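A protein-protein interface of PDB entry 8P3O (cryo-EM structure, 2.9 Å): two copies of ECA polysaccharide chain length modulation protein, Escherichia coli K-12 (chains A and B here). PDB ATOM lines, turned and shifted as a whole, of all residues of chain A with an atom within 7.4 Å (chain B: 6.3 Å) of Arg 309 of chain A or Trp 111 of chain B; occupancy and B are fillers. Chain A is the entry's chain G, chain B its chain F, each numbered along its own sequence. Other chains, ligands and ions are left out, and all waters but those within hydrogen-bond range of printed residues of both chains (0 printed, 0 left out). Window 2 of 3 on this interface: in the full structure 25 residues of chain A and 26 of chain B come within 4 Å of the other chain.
OG1 of Thr 310 of chain A lies within hydrogen-bond range of OD2 of Asp 112 of chain B (3.0 Å).
O of Leu 308 of chain A lies within hydrogen-bond range of OG of Ser 110 of chain B.
NE of Arg 114 of chain B lies within hydrogen-bond range of O of Ser 110 of chain B (3.5 Å).
O of Ile 60 of chain A lies within hydrogen-bond range of N of Arg 309 of chain A (3.4 Å).
The side-chain hydroxyl (OG) of Ser 110 of chain B sits close to the backbone NH (N) of Asp 112 of chain B, 3.2 Å away.
The backbone carbonyl oxygen (O) of Ile 60 of chain A is in hydrogen-bond range of the backbone NH (N) of Leu 308 of chain A (2.9 Å).
Leu 308 of chain A touches Trp 111 of chain B (O to N, 3.7 Å).
Leu 308 of chain A touches Asp 112 of chain B.
Arg 309 of chain A touches Trp 111 of chain B.
Asp 112 of chain B touches Arg 309 of chain A.
Leu 175 of chain A touches none of the printed residues of chain B.
Of the printed residues of chain B, Leu 308 of chain A touches Ser 110, Trp 111 and Asp 112.
Of the printed residues of chain B, Thr 310 of chain A touches Asp 112 (3.0 Å).
Glu 312 of chain A touches none of the printed residues of chain B.
Of the printed residues of chain A, Ser 110 of chain B touches Leu 308.
Trp 111 of chain B touches just these residues of chain A: Leu 308 (3.7 Å) and Arg 309 (3.8 Å).
Of the printed residues of chain A, Asp 112 of chain B touches Leu 308, Arg 309 and Thr 310.
The nearest printed residue of chain B that does not touch Arg 309 of chain A is Ser 110 of chain B (5.2 Å).
Of the 13 printed residues of chain B, 3 touch a printed residue of chain A.
Printed residues of chain B that touch a printed residue of chain A: Ser 110, Trp 111 and Asp 112.
Hydrophobic or aromatic side chains of chain B within 4 Å of the printed part of chain A: Trp 111.
Along chain B the printed residues that touch a printed residue of chain A span positions 110 to 112.
Among the printed residues, no Asp or Glu carboxylate lies within 4 Å of a Lys or Arg side-chain nitrogen of the other chain.
No position is printed for both chains.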
ATOM      1  N   SER A  57     -27.941 -19.556   4.854  1.00  0.00           N
ATOM      2  CA  SER A  57     -27.147 -18.422   5.304  1.00  0.00           C
ATOM      3  C   SER A  57     -26.082 -18.135   4.255  1.00  0.00           C
ATOM      4  O   SER A  57     -25.766 -18.984   3.419  1.00  0.00           O
ATOM      5  CB  SER A  57     -26.504 -18.686   6.669  1.00  0.00           C
ATOM      6  OG  SER A  57     -27.374 -18.316   7.722  1.00  0.00           O
ATOM      7  N   THR A  58     -25.525 -16.926   4.306  1.00  0.00           N
ATOM      8  CA  THR A  58     -24.582 -16.479   3.292  1.00  0.00           C
ATOM      9  C   THR A  58     -23.523 -15.586   3.925  1.00  0.00           C
ATOM     10  O   THR A  58     -23.739 -14.996   4.985  1.00  0.00           O
ATOM     11  CB  THR A  58     -25.294 -15.719   2.160  1.00  0.00           C
ATOM     12  OG1 THR A  58     -26.570 -16.319   1.909  1.00  0.00           O
ATOM     13  CG2 THR A  58     -24.472 -15.761   0.881  1.00  0.00           C
ATOM     14  N   ALA A  59     -22.373 -15.495   3.258  1.00  0.00           N
ATOM     15  CA  ALA A  59     -21.289 -14.625   3.688  1.00  0.00           C
ATOM     16  C   ALA A  59     -20.428 -14.273   2.485  1.00  0.00           C
ATOM     17  O   ALA A  59     -20.329 -15.043   1.528  1.00  0.00           O
ATOM     18  CB  ALA A  59     -20.436 -15.281   4.780  1.00  0.00           C
ATOM     19  N   ILE A  60     -19.801 -13.099   2.547  1.00  0.00           N
ATOM     20  CA  ILE A  60     -18.924 -12.606   1.493  1.00  0.00           C
ATOM     21  C   ILE A  60     -17.658 -12.064   2.140  1.00  0.00           C
ATOM     22  O   ILE A  60     -17.722 -11.372   3.162  1.00  0.00           O
ATOM     23  CB  ILE A  60     -19.610 -11.521   0.636  1.00  0.00           C
ATOM     24  CG1 ILE A  60     -20.902 -12.058   0.019  1.00  0.00           C
ATOM     25  CG2 ILE A  60     -18.678 -11.032  -0.458  1.00  0.00           C
ATOM     26  CD1 ILE A  60     -21.574 -11.092  -0.927  1.00  0.00           C
ATOM     27  N   THR A  61     -16.508 -12.377   1.545  1.00  0.00           N
ATOM     28  CA  THR A  61     -15.214 -12.051   2.127  1.00  0.00           C
ATOM     29  C   THR A  61     -14.338 -11.340   1.106  1.00  0.00           C
ATOM     30  O   THR A  61     -14.638 -11.309  -0.090  1.00  0.00           O
ATOM     31  CB  THR A  61     -14.494 -13.309   2.632  1.00  0.00           C
ATOM     32  OG1 THR A  61     -14.372 -14.251   1.559  1.00  0.00           O
ATOM     33  CG2 THR A  61     -15.268 -13.947   3.775  1.00  0.00           C
ATOM     34  N   LEU A 175     -22.265 -21.425  10.315  1.00  0.00           N
ATOM     35  CA  LEU A 175     -21.501 -20.727   9.286  1.00  0.00           C
ATOM     36  C   LEU A 175     -20.405 -19.861   9.891  1.00  0.00           C
ATOM     37  O   LEU A 175     -19.321 -19.743   9.308  1.00  0.00           O
ATOM     38  CB  LEU A 175     -22.430 -19.876   8.424  1.00  0.00           C
ATOM     39  CG  LEU A 175     -21.789 -19.220   7.200  1.00  0.00           C
ATOM     40  CD1 LEU A 175     -20.960 -20.225   6.421  1.00  0.00           C
ATOM     41  CD2 LEU A 175     -22.845 -18.590   6.311  1.00  0.00           C
ATOM     42  N   ARG A 306     -11.440 -10.625   5.589  1.00  0.00           N
ATOM     43  CA  ARG A 306     -12.285  -9.612   6.204  1.00  0.00           C
ATOM     44  C   ARG A 306     -13.687  -9.734   5.625  1.00  0.00           C
ATOM     45  O   ARG A 306     -13.881 -10.222   4.510  1.00  0.00           O
ATOM     46  CB  ARG A 306     -11.723  -8.199   6.003  1.00  0.00           C
ATOM     47  CG  ARG A 306     -12.032  -7.562   4.662  1.00  0.00           C
ATOM     48  CD  ARG A 306     -11.552  -6.120   4.653  1.00  0.00           C
ATOM     49  NE  ARG A 306     -11.612  -5.514   3.330  1.00  0.00           N
ATOM     50  CZ  ARG A 306     -11.948  -4.251   3.105  1.00  0.00           C
ATOM     51  NH1 ARG A 306     -12.264  -3.432   4.094  1.00  0.00           N
ATOM     52  NH2 ARG A 306     -11.965  -3.796   1.855  1.00  0.00           N
ATOM     53  N   TYR A 307     -14.667  -9.280   6.402  1.00  0.00           N
ATOM     54  CA  TYR A 307     -16.071  -9.507   6.092  1.00  0.00           C
ATOM     55  C   TYR A 307     -16.644  -8.369   5.258  1.00  0.00           C
ATOM     56  O   TYR A 307     -16.416  -7.192   5.556  1.00  0.00           O
ATOM     57  CB  TYR A 307     -16.883  -9.661   7.378  1.00  0.00           C
ATOM     58  CG  TYR A 307     -17.080 -11.090   7.818  1.00  0.00           C
ATOM     59  CD1 TYR A 307     -17.376 -12.084   6.898  1.00  0.00           C
ATOM     60  CD2 TYR A 307     -16.982 -11.444   9.157  1.00  0.00           C
ATOM     61  CE1 TYR A 307     -17.561 -13.391   7.295  1.00  0.00           C
ATOM     62  CE2 TYR A 307     -17.166 -12.748   9.564  1.00  0.00           C
ATOM     63  CZ  TYR A 307     -17.456 -13.718   8.630  1.00  0.00           C
ATOM     64  OH  TYR A 307     -17.640 -15.019   9.031  1.00  0.00           O
ATOM     65  N   LEU A 308     -17.391  -8.730   4.214  1.00  0.00           N
ATOM     66  CA  LEU A 308     -18.238  -7.783   3.501  1.00  0.00           C
ATOM     67  C   LEU A 308     -19.719  -8.024   3.745  1.00  0.00           C
ATOM     68  O   LEU A 308     -20.531  -7.134   3.471  1.00  0.00           O
ATOM     69  CB  LEU A 308     -17.960  -7.837   1.995  1.00  0.00           C
ATOM     70  CG  LEU A 308     -16.615  -7.273   1.536  1.00  0.00           C
ATOM     71  CD1 LEU A 308     -16.535  -7.244   0.018  1.00  0.00           C
ATOM     72  CD2 LEU A 308     -16.398  -5.886   2.111  1.00  0.00           C
ATOM     73  N   ARG A 309     -20.086  -9.200   4.252  1.00  0.00           N
ATOM     74  CA  ARG A 309     -21.464  -9.487   4.636  1.00  0.00           C
ATOM     75  C   ARG A 309     -21.424 -10.554   5.720  1.00  0.00           C
ATOM     76  O   ARG A 309     -21.182 -11.727   5.427  1.00  0.00           O
ATOM     77  CB  ARG A 309     -22.295  -9.947   3.442  1.00  0.00           C
ATOM     78  CG  ARG A 309     -23.656 -10.492   3.830  1.00  0.00           C
ATOM     79  CD  ARG A 309     -24.433 -10.977   2.624  1.00  0.00           C
ATOM     80  NE  ARG A 309     -25.744 -11.487   3.007  1.00  0.00           N
ATOM     81  CZ  ARG A 309     -26.743 -11.699   2.162  1.00  0.00           C
ATOM     82  NH1 ARG A 309     -26.617 -11.453   0.868  1.00  0.00           N
ATOM     83  NH2 ARG A 309     -27.897 -12.168   2.628  1.00  0.00           N
ATOM     84  N   THR A 310     -21.650 -10.146   6.959  1.00  0.00           N
ATOM     85  CA  THR A 310     -21.629 -11.082   8.076  1.00  0.00           C
ATOM     86  C   THR A 310     -22.840 -12.011   8.002  1.00  0.00           C
ATOM     87  O   THR A 310     -23.935 -11.573   7.643  1.00  0.00           O
ATOM     88  CB  THR A 310     -21.634 -10.321   9.402  1.00  0.00           C
ATOM     89  OG1 THR A 310     -20.671  -9.262   9.346  1.00  0.00           O
ATOM     90  CG2 THR A 310     -21.285 -11.243  10.558  1.00  0.00           C
ATOM     91  N   PRO A 311     -22.670 -13.295   8.320  1.00  0.00           N
ATOM     92  CA  PRO A 311     -23.825 -14.200   8.351  1.00  0.00           C
ATOM     93  C   PRO A 311     -24.857 -13.749   9.374  1.00  0.00           C
ATOM     94  O   PRO A 311     -24.528 -13.192  10.423  1.00  0.00           O
ATOM     95  CB  PRO A 311     -23.209 -15.547   8.737  1.00  0.00           C
ATOM     96  CG  PRO A 311     -21.803 -15.461   8.274  1.00  0.00           C
ATOM     97  CD  PRO A 311     -21.394 -14.023   8.427  1.00  0.00           C
ATOM     98  N   GLU A 312     -26.124 -13.999   9.051  1.00  0.00           N
ATOM     99  CA  GLU A 312     -27.229 -13.590   9.905  1.00  0.00           C
ATOM    100  C   GLU A 312     -28.357 -14.603   9.783  1.00  0.00           C
ATOM    101  O   GLU A 312     -28.405 -15.398   8.841  1.00  0.00           O
ATOM    102  CB  GLU A 312     -27.726 -12.185   9.549  1.00  0.00           C
ATOM    103  CG  GLU A 312     -27.942 -11.285  10.753  1.00  0.00           C
ATOM    104  CD  GLU A 312     -26.644 -10.731  11.306  1.00  0.00           C
ATOM    105  OE1 GLU A 312     -25.878 -10.122  10.529  1.00  0.00           O
ATOM    106  OE2 GLU A 312     -26.391 -10.902  12.516  1.00  0.00           O
ATOM    107  N   GLN B 107     -17.356   0.287   0.095  1.00  0.00           N
ATOM    108  CA  GLN B 107     -18.244   0.490   1.233  1.00  0.00           C
ATOM    109  C   GLN B 107     -19.663   0.819   0.793  1.00  0.00           C
ATOM    110  O   GLN B 107     -20.618   0.536   1.524  1.00  0.00           O
ATOM    111  CB  GLN B 107     -17.698   1.601   2.129  1.00  0.00           C
ATOM    112  CG  GLN B 107     -16.322   1.311   2.695  1.00  0.00           C
ATOM    113  CD  GLN B 107     -16.381   0.566   4.010  1.00  0.00           C
ATOM    114  OE1 GLN B 107     -17.390   0.607   4.714  1.00  0.00           O
ATOM    115  NE2 GLN B 107     -15.299  -0.125   4.349  1.00  0.00           N
ATOM    116  N   LEU B 108     -19.822   1.421  -0.388  1.00  0.00           N
ATOM    117  CA  LEU B 108     -21.153   1.791  -0.859  1.00  0.00           C
ATOM    118  C   LEU B 108     -22.019   0.565  -1.112  1.00  0.00           C
ATOM    119  O   LEU B 108     -23.196   0.537  -0.730  1.00  0.00           O
ATOM    120  CB  LEU B 108     -21.042   2.633  -2.129  1.00  0.00           C
ATOM    121  CG  LEU B 108     -21.959   3.851  -2.240  1.00  0.00           C
ATOM    122  CD1 LEU B 108     -21.820   4.744  -1.023  1.00  0.00           C
ATOM    123  CD2 LEU B 108     -21.658   4.626  -3.510  1.00  0.00           C
ATOM    124  N   ALA B 109     -21.459  -0.459  -1.747  1.00  0.00           N
ATOM    125  CA  ALA B 109     -22.219  -1.626  -2.172  1.00  0.00           C
ATOM    126  C   ALA B 109     -22.245  -2.703  -1.094  1.00  0.00           C
ATOM    127  O   ALA B 109     -22.890  -3.737  -1.294  1.00  0.00           O
ATOM    128  CB  ALA B 109     -21.652  -2.169  -3.486  1.00  0.00           C
ATOM    129  N   SER B 110     -21.568  -2.498   0.030  1.00  0.00           N
ATOM    130  CA  SER B 110     -21.503  -3.522   1.065  1.00  0.00           C
ATOM    131  C   SER B 110     -22.847  -3.762   1.734  1.00  0.00           C
ATOM    132  O   SER B 110     -23.567  -2.818   2.072  1.00  0.00           O
ATOM    133  CB  SER B 110     -20.485  -3.128   2.133  1.00  0.00           C
ATOM    134  OG  SER B 110     -20.430  -4.100   3.161  1.00  0.00           O
ATOM    135  N   TRP B 111     -23.188  -5.040   1.916  1.00  0.00           N
ATOM    136  CA  TRP B 111     -24.419  -5.392   2.615  1.00  0.00           C
ATOM    137  C   TRP B 111     -24.319  -4.941   4.066  1.00  0.00           C
ATOM    138  O   TRP B 111     -25.322  -4.518   4.652  1.00  0.00           O
ATOM    139  CB  TRP B 111     -24.725  -6.889   2.530  1.00  0.00           C
ATOM    140  CG  TRP B 111     -25.855  -7.364   3.402  1.00  0.00           C
ATOM    141  CD1 TRP B 111     -25.830  -7.553   4.754  1.00  0.00           C
ATOM    142  CD2 TRP B 111     -27.173  -7.730   2.975  1.00  0.00           C
ATOM    143  NE1 TRP B 111     -27.049  -8.001   5.195  1.00  0.00           N
ATOM    144  CE2 TRP B 111     -27.890  -8.119   4.122  1.00  0.00           C
ATOM    145  CE3 TRP B 111     -27.816  -7.759   1.734  1.00  0.00           C
ATOM    146  CZ2 TRP B 111     -29.217  -8.533   4.067  1.00  0.00           C
ATOM    147  CZ3 TRP B 111     -29.133  -8.171   1.681  1.00  0.00           C
ATOM    148  CH2 TRP B 111     -29.820  -8.553   2.839  1.00  0.00           C
ATOM    149  N   ASP B 112     -23.127  -5.025   4.660  1.00  0.00           N
ATOM    150  CA  ASP B 112     -22.967  -4.655   6.062  1.00  0.00           C
ATOM    151  C   ASP B 112     -23.225  -3.172   6.284  1.00  0.00           C
ATOM    152  O   ASP B 112     -23.882  -2.793   7.260  1.00  0.00           O
ATOM    153  CB  ASP B 112     -21.568  -5.034   6.544  1.00  0.00           C
ATOM    154  CG  ASP B 112     -21.544  -6.355   7.285  1.00  0.00           C
ATOM    155  OD1 ASP B 112     -22.628  -6.944   7.482  1.00  0.00           O
ATOM    156  OD2 ASP B 112     -20.446  -6.805   7.668  1.00  0.00           O
ATOM    157  N   THR B 113     -22.724  -2.317   5.388  1.00  0.00           N
ATOM    158  CA  THR B 113     -22.887  -0.877   5.566  1.00  0.00           C
ATOM    159  C   THR B 113     -24.355  -0.474   5.542  1.00  0.00           C
ATOM    160  O   THR B 113     -24.785   0.372   6.335  1.00  0.00           O
ATOM    161  CB  THR B 113     -22.112  -0.120   4.489  1.00  0.00           C
ATOM    162  OG1 THR B 113     -20.774  -0.627   4.416  1.00  0.00           O
ATOM    163  CG2 THR B 113     -22.066   1.363   4.811  1.00  0.00           C
ATOM    164  N   ARG B 114     -25.137  -1.064   4.635  1.00  0.00           N
ATOM    165  CA  ARG B 114     -26.560  -0.751   4.571  1.00  0.00           C
ATOM    166  C   ARG B 114     -27.291  -1.174   5.838  1.00  0.00           C
ATOM    167  O   ARG B 114     -28.291  -0.551   6.209  1.00  0.00           O
ATOM    168  CB  ARG B 114     -27.187  -1.415   3.348  1.00  0.00           C
ATOM    169  CG  ARG B 114     -26.775  -0.788   2.028  1.00  0.00           C
ATOM    170  CD  ARG B 114     -27.408  -1.500   0.847  1.00  0.00           C
ATOM    171  NE  ARG B 114     -26.564  -2.571   0.335  1.00  0.00           N
ATOM    172  CZ  ARG B 114     -26.996  -3.568  -0.425  1.00  0.00           C
ATOM    173  NH1 ARG B 114     -28.266  -3.667  -0.778  1.00  0.00           N
ATOM    174  NH2 ARG B 114     -26.131  -4.487  -0.842  1.00  0.00           N
ATOM    175  N   ARG B 115     -26.818  -2.224   6.509  1.00  0.00           N
ATOM    176  CA  ARG B 115     -27.499  -2.698   7.709  1.00  0.00           C
ATOM    177  C   ARG B 115     -27.267  -1.771   8.896  1.00  0.00           C
ATOM    178  O   ARG B 115     -28.196  -1.501   9.665  1.00  0.00           O
ATOM    179  CB  ARG B 115     -27.045  -4.118   8.046  1.00  0.00           C
ATOM    180  CG  ARG B 115     -27.852  -4.772   9.152  1.00  0.00           C
ATOM    181  CD  ARG B 115     -27.456  -6.223   9.345  1.00  0.00           C
ATOM    182  NE  ARG B 115     -28.322  -6.900  10.304  1.00  0.00           N
ATOM    183  CZ  ARG B 115     -28.183  -6.825  11.619  1.00  0.00           C
ATOM    184  NH1 ARG B 115     -27.219  -6.106  12.172  1.00  0.00           N
ATOM    185  NH2 ARG B 115     -29.031  -7.486  12.402  1.00  0.00           N
ATOM    186  N   GLU B 116     -26.039  -1.279   9.068  1.00  0.00           N
ATOM    187  CA  GLU B 116     -25.747  -0.368  10.167  1.00  0.00           C
ATOM    188  C   GLU B 116     -26.395   0.997   9.988  1.00  0.00           C
ATOM    189  O   GLU B 116     -26.710   1.652  10.987  1.00  0.00           O
ATOM    190  CB  GLU B 116     -24.235  -0.189  10.327  1.00  0.00           C
ATOM    191  CG  GLU B 116     -23.419  -1.424  10.007  1.00  0.00           C
ATOM    192  CD  GLU B 116     -23.352  -2.393  11.168  1.00  0.00           C
ATOM    193  OE1 GLU B 116     -23.754  -2.007  12.287  1.00  0.00           O
ATOM    194  OE2 GLU B 116     -22.899  -3.539  10.965  1.00  0.00           O
ATOM    195  N   ASP B 140     -35.003  -6.433   6.633  1.00  0.00           N
ATOM    196  CA  ASP B 140     -34.474  -7.042   5.417  1.00  0.00           C
ATOM    197  C   ASP B 140     -35.080  -6.424   4.166  1.00  0.00           C
ATOM    198  O   ASP B 140     -34.426  -6.381   3.116  1.00  0.00           O
ATOM    199  CB  ASP B 140     -34.717  -8.550   5.435  1.00  0.00           C
ATOM    200  CG  ASP B 140     -33.565  -9.331   4.839  1.00  0.00           C
ATOM    201  OD1 ASP B 140     -32.848  -8.774   3.981  1.00  0.00           O
ATOM    202  OD2 ASP B 140     -33.374 -10.502   5.228  1.00  0.00           O
ATOM    203  N   ILE B 143     -33.132  -3.123   3.351  1.00  0.00           N
ATOM    204  CA  ILE B 143     -31.786  -3.289   2.805  1.00  0.00           C
ATOM    205  C   ILE B 143     -31.829  -3.355   1.283  1.00  0.00           C
ATOM    206  O   ILE B 143     -30.912  -2.885   0.600  1.00  0.00           O
ATOM    207  CB  ILE B 143     -31.112  -4.534   3.408  1.00  0.00           C
ATOM    208  CG1 ILE B 143     -31.210  -4.508   4.932  1.00  0.00           C
ATOM    209  CG2 ILE B 143     -29.660  -4.620   2.975  1.00  0.00           C
ATOM    210  CD1 ILE B 143     -30.381  -3.426   5.572  1.00  0.00           C
ATOM    211  N   ASN B 144     -32.892  -3.934   0.729  1.00  0.00           N
ATOM    212  CA  ASN B 144     -33.020  -4.059  -0.717  1.00  0.00           C
ATOM    213  C   ASN B 144     -33.537  -2.792  -1.381  1.00  0.00           C
ATOM    214  O   ASN B 144     -33.660  -2.764  -2.611  1.00  0.00           O
ATOM    215  CB  ASN B 144     -33.941  -5.229  -1.064  1.00  0.00           C
ATOM    216  CG  ASN B 144     -33.335  -6.569  -0.710  1.00  0.00           C
ATOM    217  OD1 ASN B 144     -33.823  -7.269   0.178  1.00  0.00           O
ATOM    218  ND2 ASN B 144     -32.263  -6.935  -1.402  1.00  0.00           N
